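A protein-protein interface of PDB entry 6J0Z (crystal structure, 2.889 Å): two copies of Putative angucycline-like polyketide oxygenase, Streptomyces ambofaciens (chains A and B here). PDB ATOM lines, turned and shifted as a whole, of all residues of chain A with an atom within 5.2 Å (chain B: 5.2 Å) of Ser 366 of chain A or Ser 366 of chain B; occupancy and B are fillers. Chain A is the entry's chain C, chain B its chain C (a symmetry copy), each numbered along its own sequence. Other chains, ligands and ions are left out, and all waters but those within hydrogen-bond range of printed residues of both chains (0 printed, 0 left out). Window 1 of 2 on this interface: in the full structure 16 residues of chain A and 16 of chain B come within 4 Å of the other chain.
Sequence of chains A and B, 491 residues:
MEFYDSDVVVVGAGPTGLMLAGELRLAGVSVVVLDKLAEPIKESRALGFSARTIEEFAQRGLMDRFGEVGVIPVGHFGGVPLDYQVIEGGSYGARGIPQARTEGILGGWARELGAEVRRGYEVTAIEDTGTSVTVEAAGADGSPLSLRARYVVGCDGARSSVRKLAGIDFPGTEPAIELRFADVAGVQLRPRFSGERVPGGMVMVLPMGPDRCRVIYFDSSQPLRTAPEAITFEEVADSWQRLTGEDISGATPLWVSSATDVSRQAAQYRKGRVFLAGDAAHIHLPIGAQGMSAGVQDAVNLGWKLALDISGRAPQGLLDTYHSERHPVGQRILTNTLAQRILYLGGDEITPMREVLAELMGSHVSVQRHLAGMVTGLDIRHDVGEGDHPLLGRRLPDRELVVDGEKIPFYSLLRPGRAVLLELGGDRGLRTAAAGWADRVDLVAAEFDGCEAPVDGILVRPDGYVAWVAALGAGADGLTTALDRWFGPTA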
ATOM      1  N   LEU A 360      -4.360  -0.869 -16.289  1.00  0.00           N
ATOM      2  CA  LEU A 360      -3.154  -0.473 -15.574  1.00  0.00           C
ATOM      3  C   LEU A 360      -3.461   0.117 -14.203  1.00  0.00           C
ATOM      4  O   LEU A 360      -2.647  -0.033 -13.281  1.00  0.00           O
ATOM      5  CB  LEU A 360      -2.370   0.529 -16.424  1.00  0.00           C
ATOM      6  CG  LEU A 360      -1.793   0.000 -17.736  1.00  0.00           C
ATOM      7  CD1 LEU A 360      -1.173   1.128 -18.547  1.00  0.00           C
ATOM      8  CD2 LEU A 360      -0.779  -1.077 -17.428  1.00  0.00           C
ATOM      9  N   MET A 361      -4.615   0.784 -14.048  1.00  0.00           N
ATOM     10  CA  MET A 361      -5.021   1.335 -12.757  1.00  0.00           C
ATOM     11  C   MET A 361      -5.362   0.262 -11.741  1.00  0.00           C
ATOM     12  O   MET A 361      -5.500   0.587 -10.555  1.00  0.00           O
ATOM     13  CB  MET A 361      -6.258   2.233 -12.844  1.00  0.00           C
ATOM     14  CG  MET A 361      -6.242   3.426 -13.759  1.00  0.00           C
ATOM     15  SD  MET A 361      -4.718   4.349 -13.874  1.00  0.00           S
ATOM     16  CE  MET A 361      -4.285   4.658 -12.177  1.00  0.00           C
ATOM     17  N   SER A 363      -3.303  -1.781 -10.864  1.00  0.00           N
ATOM     18  CA  SER A 363      -2.072  -1.760 -10.107  1.00  0.00           C
ATOM     19  C   SER A 363      -1.901  -0.432  -9.395  1.00  0.00           C
ATOM     20  O   SER A 363      -2.152   0.628  -9.971  1.00  0.00           O
ATOM     21  CB  SER A 363      -0.895  -1.976 -11.037  1.00  0.00           C
ATOM     22  OG  SER A 363      -1.160  -3.061 -11.920  1.00  0.00           O
ATOM     23  N   HIS A 364      -1.438  -0.500  -8.136  1.00  0.00           N
ATOM     24  CA  HIS A 364      -1.318   0.725  -7.357  1.00  0.00           C
ATOM     25  C   HIS A 364      -0.036   1.500  -7.585  1.00  0.00           C
ATOM     26  O   HIS A 364       0.021   2.683  -7.236  1.00  0.00           O
ATOM     27  CB  HIS A 364      -1.487   0.394  -5.875  1.00  0.00           C
ATOM     28  CG  HIS A 364      -2.894   0.037  -5.518  1.00  0.00           C
ATOM     29  ND1 HIS A 364      -3.971   0.806  -5.912  1.00  0.00           N
ATOM     30  CD2 HIS A 364      -3.408  -1.022  -4.850  1.00  0.00           C
ATOM     31  CE1 HIS A 364      -5.087   0.243  -5.485  1.00  0.00           C
ATOM     32  NE2 HIS A 364      -4.774  -0.867  -4.839  1.00  0.00           N
ATOM     33  N   VAL A 365       0.958   0.899  -8.187  1.00  0.00           N
ATOM     34  CA  VAL A 365       2.079   1.709  -8.626  1.00  0.00           C
ATOM     35  C   VAL A 365       1.612   2.677  -9.709  1.00  0.00           C
ATOM     36  O   VAL A 365       1.932   3.871  -9.680  1.00  0.00           O
ATOM     37  CB  VAL A 365       3.234   0.809  -9.087  1.00  0.00           C
ATOM     38  CG1 VAL A 365       4.471   1.635  -9.194  1.00  0.00           C
ATOM     39  CG2 VAL A 365       3.449  -0.305  -8.075  1.00  0.00           C
ATOM     40  N   SER A 366       0.790   2.192 -10.646  1.00  0.00           N
ATOM     41  CA  SER A 366       0.194   3.079 -11.642  1.00  0.00           C
ATOM     42  C   SER A 366      -0.747   4.079 -10.994  1.00  0.00           C
ATOM     43  O   SER A 366      -0.808   5.240 -11.420  1.00  0.00           O
ATOM     44  CB  SER A 366      -0.558   2.273 -12.698  1.00  0.00           C
ATOM     45  OG  SER A 366       0.296   1.332 -13.321  1.00  0.00           O
ATOM     46  N   VAL A 367      -1.487   3.625  -9.956  1.00  0.00           N
ATOM     47  CA  VAL A 367      -2.350   4.545  -9.230  1.00  0.00           C
ATOM     48  C   VAL A 367      -1.487   5.703  -8.777  1.00  0.00           C
ATOM     49  O   VAL A 367      -1.616   6.801  -9.309  1.00  0.00           O
ATOM     50  CB  VAL A 367      -3.070   3.819  -8.088  1.00  0.00           C
ATOM     51  CG1 VAL A 367      -3.702   4.836  -7.153  1.00  0.00           C
ATOM     52  CG2 VAL A 367      -4.115   2.850  -8.647  1.00  0.00           C
ATOM     53  N   GLN A 368      -0.522   5.473  -7.896  1.00  0.00           N
ATOM     54  CA  GLN A 368       0.310   6.546  -7.367  1.00  0.00           C
ATOM     55  C   GLN A 368       0.998   7.385  -8.428  1.00  0.00           C
ATOM     56  O   GLN A 368       1.174   8.595  -8.252  1.00  0.00           O
ATOM     57  CB  GLN A 368       1.362   5.967  -6.433  1.00  0.00           C
ATOM     58  CG  GLN A 368       0.750   5.170  -5.312  1.00  0.00           C
ATOM     59  CD  GLN A 368       1.768   4.648  -4.344  1.00  0.00           C
ATOM     60  OE1 GLN A 368       1.435   3.899  -3.422  1.00  0.00           O
ATOM     61  NE2 GLN A 368       3.019   5.038  -4.536  1.00  0.00           N
ATOM     62  N   ARG A 369       1.391   6.761  -9.538  1.00  0.00           N
ATOM     63  CA  ARG A 369       2.021   7.505 -10.622  1.00  0.00           C
ATOM     64  C   ARG A 369       1.076   8.558 -11.196  1.00  0.00           C
ATOM     65  O   ARG A 369       1.428   9.740 -11.306  1.00  0.00           O
ATOM     66  CB  ARG A 369       2.418   6.536 -11.727  1.00  0.00           C
ATOM     67  CG  ARG A 369       3.084   7.227 -12.885  1.00  0.00           C
ATOM     68  CD  ARG A 369       4.280   7.933 -12.386  1.00  0.00           C
ATOM     69  NE  ARG A 369       5.047   8.575 -13.428  1.00  0.00           N
ATOM     70  CZ  ARG A 369       4.596   9.604 -14.131  1.00  0.00           C
ATOM     71  NH1 ARG A 369       3.376  10.077 -13.885  1.00  0.00           N
ATOM     72  NH2 ARG A 369       5.359  10.187 -15.022  1.00  0.00           N
ATOM     73  N   HIS A 370      -0.139   8.143 -11.553  1.00  0.00           N
ATOM     74  CA  HIS A 370      -1.111   9.075 -12.114  1.00  0.00           C
ATOM     75  C   HIS A 370      -1.606  10.057 -11.064  1.00  0.00           C
ATOM     76  O   HIS A 370      -1.906  11.221 -11.380  1.00  0.00           O
ATOM     77  CB  HIS A 370      -2.287   8.293 -12.675  1.00  0.00           C
ATOM     78  CG  HIS A 370      -2.099   7.868 -14.089  1.00  0.00           C
ATOM     79  ND1 HIS A 370      -2.861   6.876 -14.667  1.00  0.00           N
ATOM     80  CD2 HIS A 370      -1.244   8.300 -15.044  1.00  0.00           C
ATOM     81  CE1 HIS A 370      -2.481   6.716 -15.922  1.00  0.00           C
ATOM     82  NE2 HIS A 370      -1.502   7.568 -16.175  1.00  0.00           N
ATOM     83  N   LEU A 371      -1.552   9.562  -9.828  1.00  0.00           N
ATOM     84  CA  LEU A 371      -1.911  10.364  -8.645  1.00  0.00           C
ATOM     85  C   LEU A 371      -1.053  11.608  -8.646  1.00  0.00           C
ATOM     86  O   LEU A 371      -1.581  12.738  -8.662  1.00  0.00           O
ATOM     87  CB  LEU A 371      -1.505   9.503  -7.451  1.00  0.00           C
ATOM     88  CG  LEU A 371      -2.561   8.461  -7.156  1.00  0.00           C
ATOM     89  CD1 LEU A 371      -2.448   7.944  -5.727  1.00  0.00           C
ATOM     90  CD2 LEU A 371      -3.955   9.014  -7.412  1.00  0.00           C
ATOM     91  N   LEU B 360       5.200   4.997 -16.956  1.00  0.00           N
ATOM     92  CA  LEU B 360       4.531   3.882 -16.299  1.00  0.00           C
ATOM     93  C   LEU B 360       5.354   2.600 -16.349  1.00  0.00           C
ATOM     94  O   LEU B 360       5.263   1.783 -15.424  1.00  0.00           O
ATOM     95  CB  LEU B 360       3.162   3.664 -16.945  1.00  0.00           C
ATOM     96  CG  LEU B 360       2.141   4.787 -16.768  1.00  0.00           C
ATOM     97  CD1 LEU B 360       0.886   4.510 -17.580  1.00  0.00           C
ATOM     98  CD2 LEU B 360       1.822   4.933 -15.298  1.00  0.00           C
ATOM     99  N   MET B 361       6.155   2.408 -17.409  1.00  0.00           N
ATOM    100  CA  MET B 361       7.023   1.237 -17.518  1.00  0.00           C
ATOM    101  C   MET B 361       8.155   1.251 -16.510  1.00  0.00           C
ATOM    102  O   MET B 361       8.820   0.219 -16.348  1.00  0.00           O
ATOM    103  CB  MET B 361       7.689   1.103 -18.889  1.00  0.00           C
ATOM    104  CG  MET B 361       6.833   1.036 -20.123  1.00  0.00           C
ATOM    105  SD  MET B 361       5.308   0.115 -20.012  1.00  0.00           S
ATOM    106  CE  MET B 361       5.808  -1.445 -19.320  1.00  0.00           C
ATOM    107  N   SER B 363       7.604   1.274 -13.530  1.00  0.00           N
ATOM    108  CA  SER B 363       7.046   0.351 -12.566  1.00  0.00           C
ATOM    109  C   SER B 363       6.921  -1.037 -13.162  1.00  0.00           C
ATOM    110  O   SER B 363       6.499  -1.196 -14.308  1.00  0.00           O
ATOM    111  CB  SER B 363       5.674   0.829 -12.136  1.00  0.00           C
ATOM    112  OG  SER B 363       5.709   2.221 -11.840  1.00  0.00           O
ATOM    113  N   HIS B 364       7.266  -2.052 -12.352  1.00  0.00           N
ATOM    114  CA  HIS B 364       7.247  -3.413 -12.873  1.00  0.00           C
ATOM    115  C   HIS B 364       5.892  -4.091 -12.831  1.00  0.00           C
ATOM    116  O   HIS B 364       5.700  -5.091 -13.529  1.00  0.00           O
ATOM    117  CB  HIS B 364       8.287  -4.248 -12.128  1.00  0.00           C
ATOM    118  CG  HIS B 364       9.691  -3.886 -12.494  1.00  0.00           C
ATOM    119  ND1 HIS B 364      10.101  -3.761 -13.806  1.00  0.00           N
ATOM    120  CD2 HIS B 364      10.765  -3.577 -11.730  1.00  0.00           C
ATOM    121  CE1 HIS B 364      11.373  -3.408 -13.834  1.00  0.00           C
ATOM    122  NE2 HIS B 364      11.800  -3.289 -12.588  1.00  0.00           N
ATOM    123  N   VAL B 365       4.955  -3.564 -12.086  1.00  0.00           N
ATOM    124  CA  VAL B 365       3.601  -4.062 -12.243  1.00  0.00           C
ATOM    125  C   VAL B 365       3.096  -3.729 -13.644  1.00  0.00           C
ATOM    126  O   VAL B 365       2.518  -4.578 -14.333  1.00  0.00           O
ATOM    127  CB  VAL B 365       2.698  -3.501 -11.135  1.00  0.00           C
ATOM    128  CG1 VAL B 365       1.432  -4.286 -11.106  1.00  0.00           C
ATOM    129  CG2 VAL B 365       3.404  -3.620  -9.793  1.00  0.00           C
ATOM    130  N   SER B 366       3.368  -2.506 -14.115  1.00  0.00           N
ATOM    131  CA  SER B 366       3.036  -2.151 -15.492  1.00  0.00           C
ATOM    132  C   SER B 366       3.844  -2.973 -16.482  1.00  0.00           C
ATOM    133  O   SER B 366       3.325  -3.357 -17.539  1.00  0.00           O
ATOM    134  CB  SER B 366       3.279  -0.664 -15.736  1.00  0.00           C
ATOM    135  OG  SER B 366       2.538   0.127 -14.828  1.00  0.00           O
ATOM    136  N   VAL B 367       5.124  -3.241 -16.138  1.00  0.00           N
ATOM    137  CA  VAL B 367       5.936  -4.094 -16.993  1.00  0.00           C
ATOM    138  C   VAL B 367       5.173  -5.387 -17.189  1.00  0.00           C
ATOM    139  O   VAL B 367       4.668  -5.635 -18.280  1.00  0.00           O
ATOM    140  CB  VAL B 367       7.336  -4.278 -16.398  1.00  0.00           C
ATOM    141  CG1 VAL B 367       8.053  -5.409 -17.115  1.00  0.00           C
ATOM    142  CG2 VAL B 367       8.128  -2.971 -16.483  1.00  0.00           C
ATOM    143  N   GLN B 368       4.965  -6.169 -16.138  1.00  0.00           N
ATOM    144  CA  GLN B 368       4.292  -7.456 -16.257  1.00  0.00           C
ATOM    145  C   GLN B 368       2.930  -7.392 -16.921  1.00  0.00           C
ATOM    146  O   GLN B 368       2.540  -8.316 -17.642  1.00  0.00           O
ATOM    147  CB  GLN B 368       4.145  -8.087 -14.881  1.00  0.00           C
ATOM    148  CG  GLN B 368       5.468  -8.244 -14.181  1.00  0.00           C
ATOM    149  CD  GLN B 368       5.349  -8.925 -12.851  1.00  0.00           C
ATOM    150  OE1 GLN B 368       6.330  -9.044 -12.115  1.00  0.00           O
ATOM    151  NE2 GLN B 368       4.148  -9.383 -12.530  1.00  0.00           N
ATOM    152  N   ARG B 369       2.192  -6.306 -16.694  1.00  0.00           N
ATOM    153  CA  ARG B 369       0.889  -6.149 -17.330  1.00  0.00           C
ATOM    154  C   ARG B 369       1.015  -6.105 -18.851  1.00  0.00           C
ATOM    155  O   ARG B 369       0.339  -6.853 -19.570  1.00  0.00           O
ATOM    156  CB  ARG B 369       0.249  -4.856 -16.845  1.00  0.00           C
ATOM    157  CG  ARG B 369      -1.106  -4.622 -17.451  1.00  0.00           C
ATOM    158  CD  ARG B 369      -1.975  -5.767 -17.114  1.00  0.00           C
ATOM    159  NE  ARG B 369      -3.334  -5.618 -17.583  1.00  0.00           N
ATOM    160  CZ  ARG B 369      -3.660  -5.606 -18.868  1.00  0.00           C
ATOM    161  NH1 ARG B 369      -2.702  -5.728 -19.784  1.00  0.00           N
ATOM    162  NH2 ARG B 369      -4.914  -5.530 -19.235  1.00  0.00           N
ATOM    163  N   HIS B 370       1.892  -5.239 -19.355  1.00  0.00           N
ATOM    164  CA  HIS B 370       2.082  -5.122 -20.797  1.00  0.00           C
ATOM    165  C   HIS B 370       2.765  -6.356 -21.368  1.00  0.00           C
ATOM    166  O   HIS B 370       2.493  -6.754 -22.514  1.00  0.00           O
ATOM    167  CB  HIS B 370       2.924  -3.892 -21.092  1.00  0.00           C
ATOM    168  CG  HIS B 370       2.122  -2.645 -21.245  1.00  0.00           C
ATOM    169  ND1 HIS B 370       2.689  -1.392 -21.167  1.00  0.00           N
ATOM    170  CD2 HIS B 370       0.803  -2.456 -21.478  1.00  0.00           C
ATOM    171  CE1 HIS B 370       1.748  -0.482 -21.345  1.00  0.00           C
ATOM    172  NE2 HIS B 370       0.596  -1.101 -21.535  1.00  0.00           N
ATOM    173  N   LEU B 371       3.541  -6.973 -20.478  1.00  0.00           N
ATOM    174  CA  LEU B 371       4.241  -8.232 -20.789  1.00  0.00           C
ATOM    175  C   LEU B 371       3.209  -9.243 -21.232  1.00  0.00           C
ATOM    176  O   LEU B 371       3.291  -9.776 -22.356  1.00  0.00           O
ATOM    177  CB  LEU B 371       4.824  -8.694 -19.455  1.00  0.00           C
ATOM    178  CG  LEU B 371       6.115  -7.966 -19.151  1.00  0.00           C
ATOM    179  CD1 LEU B 371       6.957  -8.730 -18.135  1.00  0.00           C
ATOM    180  CD2 LEU B 371       6.911  -7.719 -20.423  1.00  0.00           C
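OG of Ser 366 of chain B sits at hydrogen-bond distance from OG of Ser 366 of chain A (3.0 Å).
O of Leu 360 of chain A lies close to OG of Ser 366 of chain A, at 3.2 Å. The side-chain hydroxyl of Ser 366 of chain B lies close to the backbone carbonyl oxygen of Leu 360 of chain B (3.2 Å).
Leu 360 of chain A touches Arg 369 of chain B. Ser 363 of chain A touches Val 365 of chain B. Val 365 of chain A touches Ser 363 of chain B (CG1 to OG, 3.0 Å). Val 365 of chain B touches Val 365 of chain A (CG2 to CG2, 3.7 Å). Arg 369 of chain A touches Leu 360 of chain B (CG to CD2, 3.6 Å).
Ser 366 of chain A touches just one residue of chain B: Ser 366. Of chain A, only Ser 366 comes within 4 Å of Ser 366 of chain B. Printed residues of chain A within 4 Å of Val 365 of chain B: Ser 363 (3.0 Å) and Val 365 (3.7 Å). Of the printed residues of chain B, Ser 363 of chain A touches Val 365 (3.0 Å). Leu 371 of chain B touches none of the printed residues of chain A. The nearest residue of chain B that does not touch Ser 366 of chain A is Leu 360 of chain B (4.4 Å). The nearest printed residue of chain A that does not touch Leu 360 of chain B is Leu 360 of chain A (4.1 Å).
Of the 11 printed residues of chain A, 5 touch a printed residue of chain B. Hydrophobic or aromatic side chains of chain A within 4 Å of the printed part of chain B: Leu 360 and Val 365. Among the printed residues, no Asp or Glu carboxylate lies within 4 Å of a Lys or Arg side-chain nitrogen of the other chain.
Leu 360 of chain A touches Arg 369 of chain B, and with the chains exchanged Arg 369 of chain A touches Leu 360 of chain B. Ser 363 of chain A touches Val 365 of chain B, and with the chains exchanged Val 365 of chain A touches Ser 363 of chain B. Val 365 of chain B touches its own counterpart, Val 365 of chain A. Ser 366 of chain A touches its own counterpart, Ser 366 of chain B. Positions printed for both chains: 360, 361, 363, 364, 365, 366, 367, 368, 369, 370 and 371. Of the 6 pairs that touch across the chains among the printed residues, 6 have their exchanged pair printed and touching as well.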
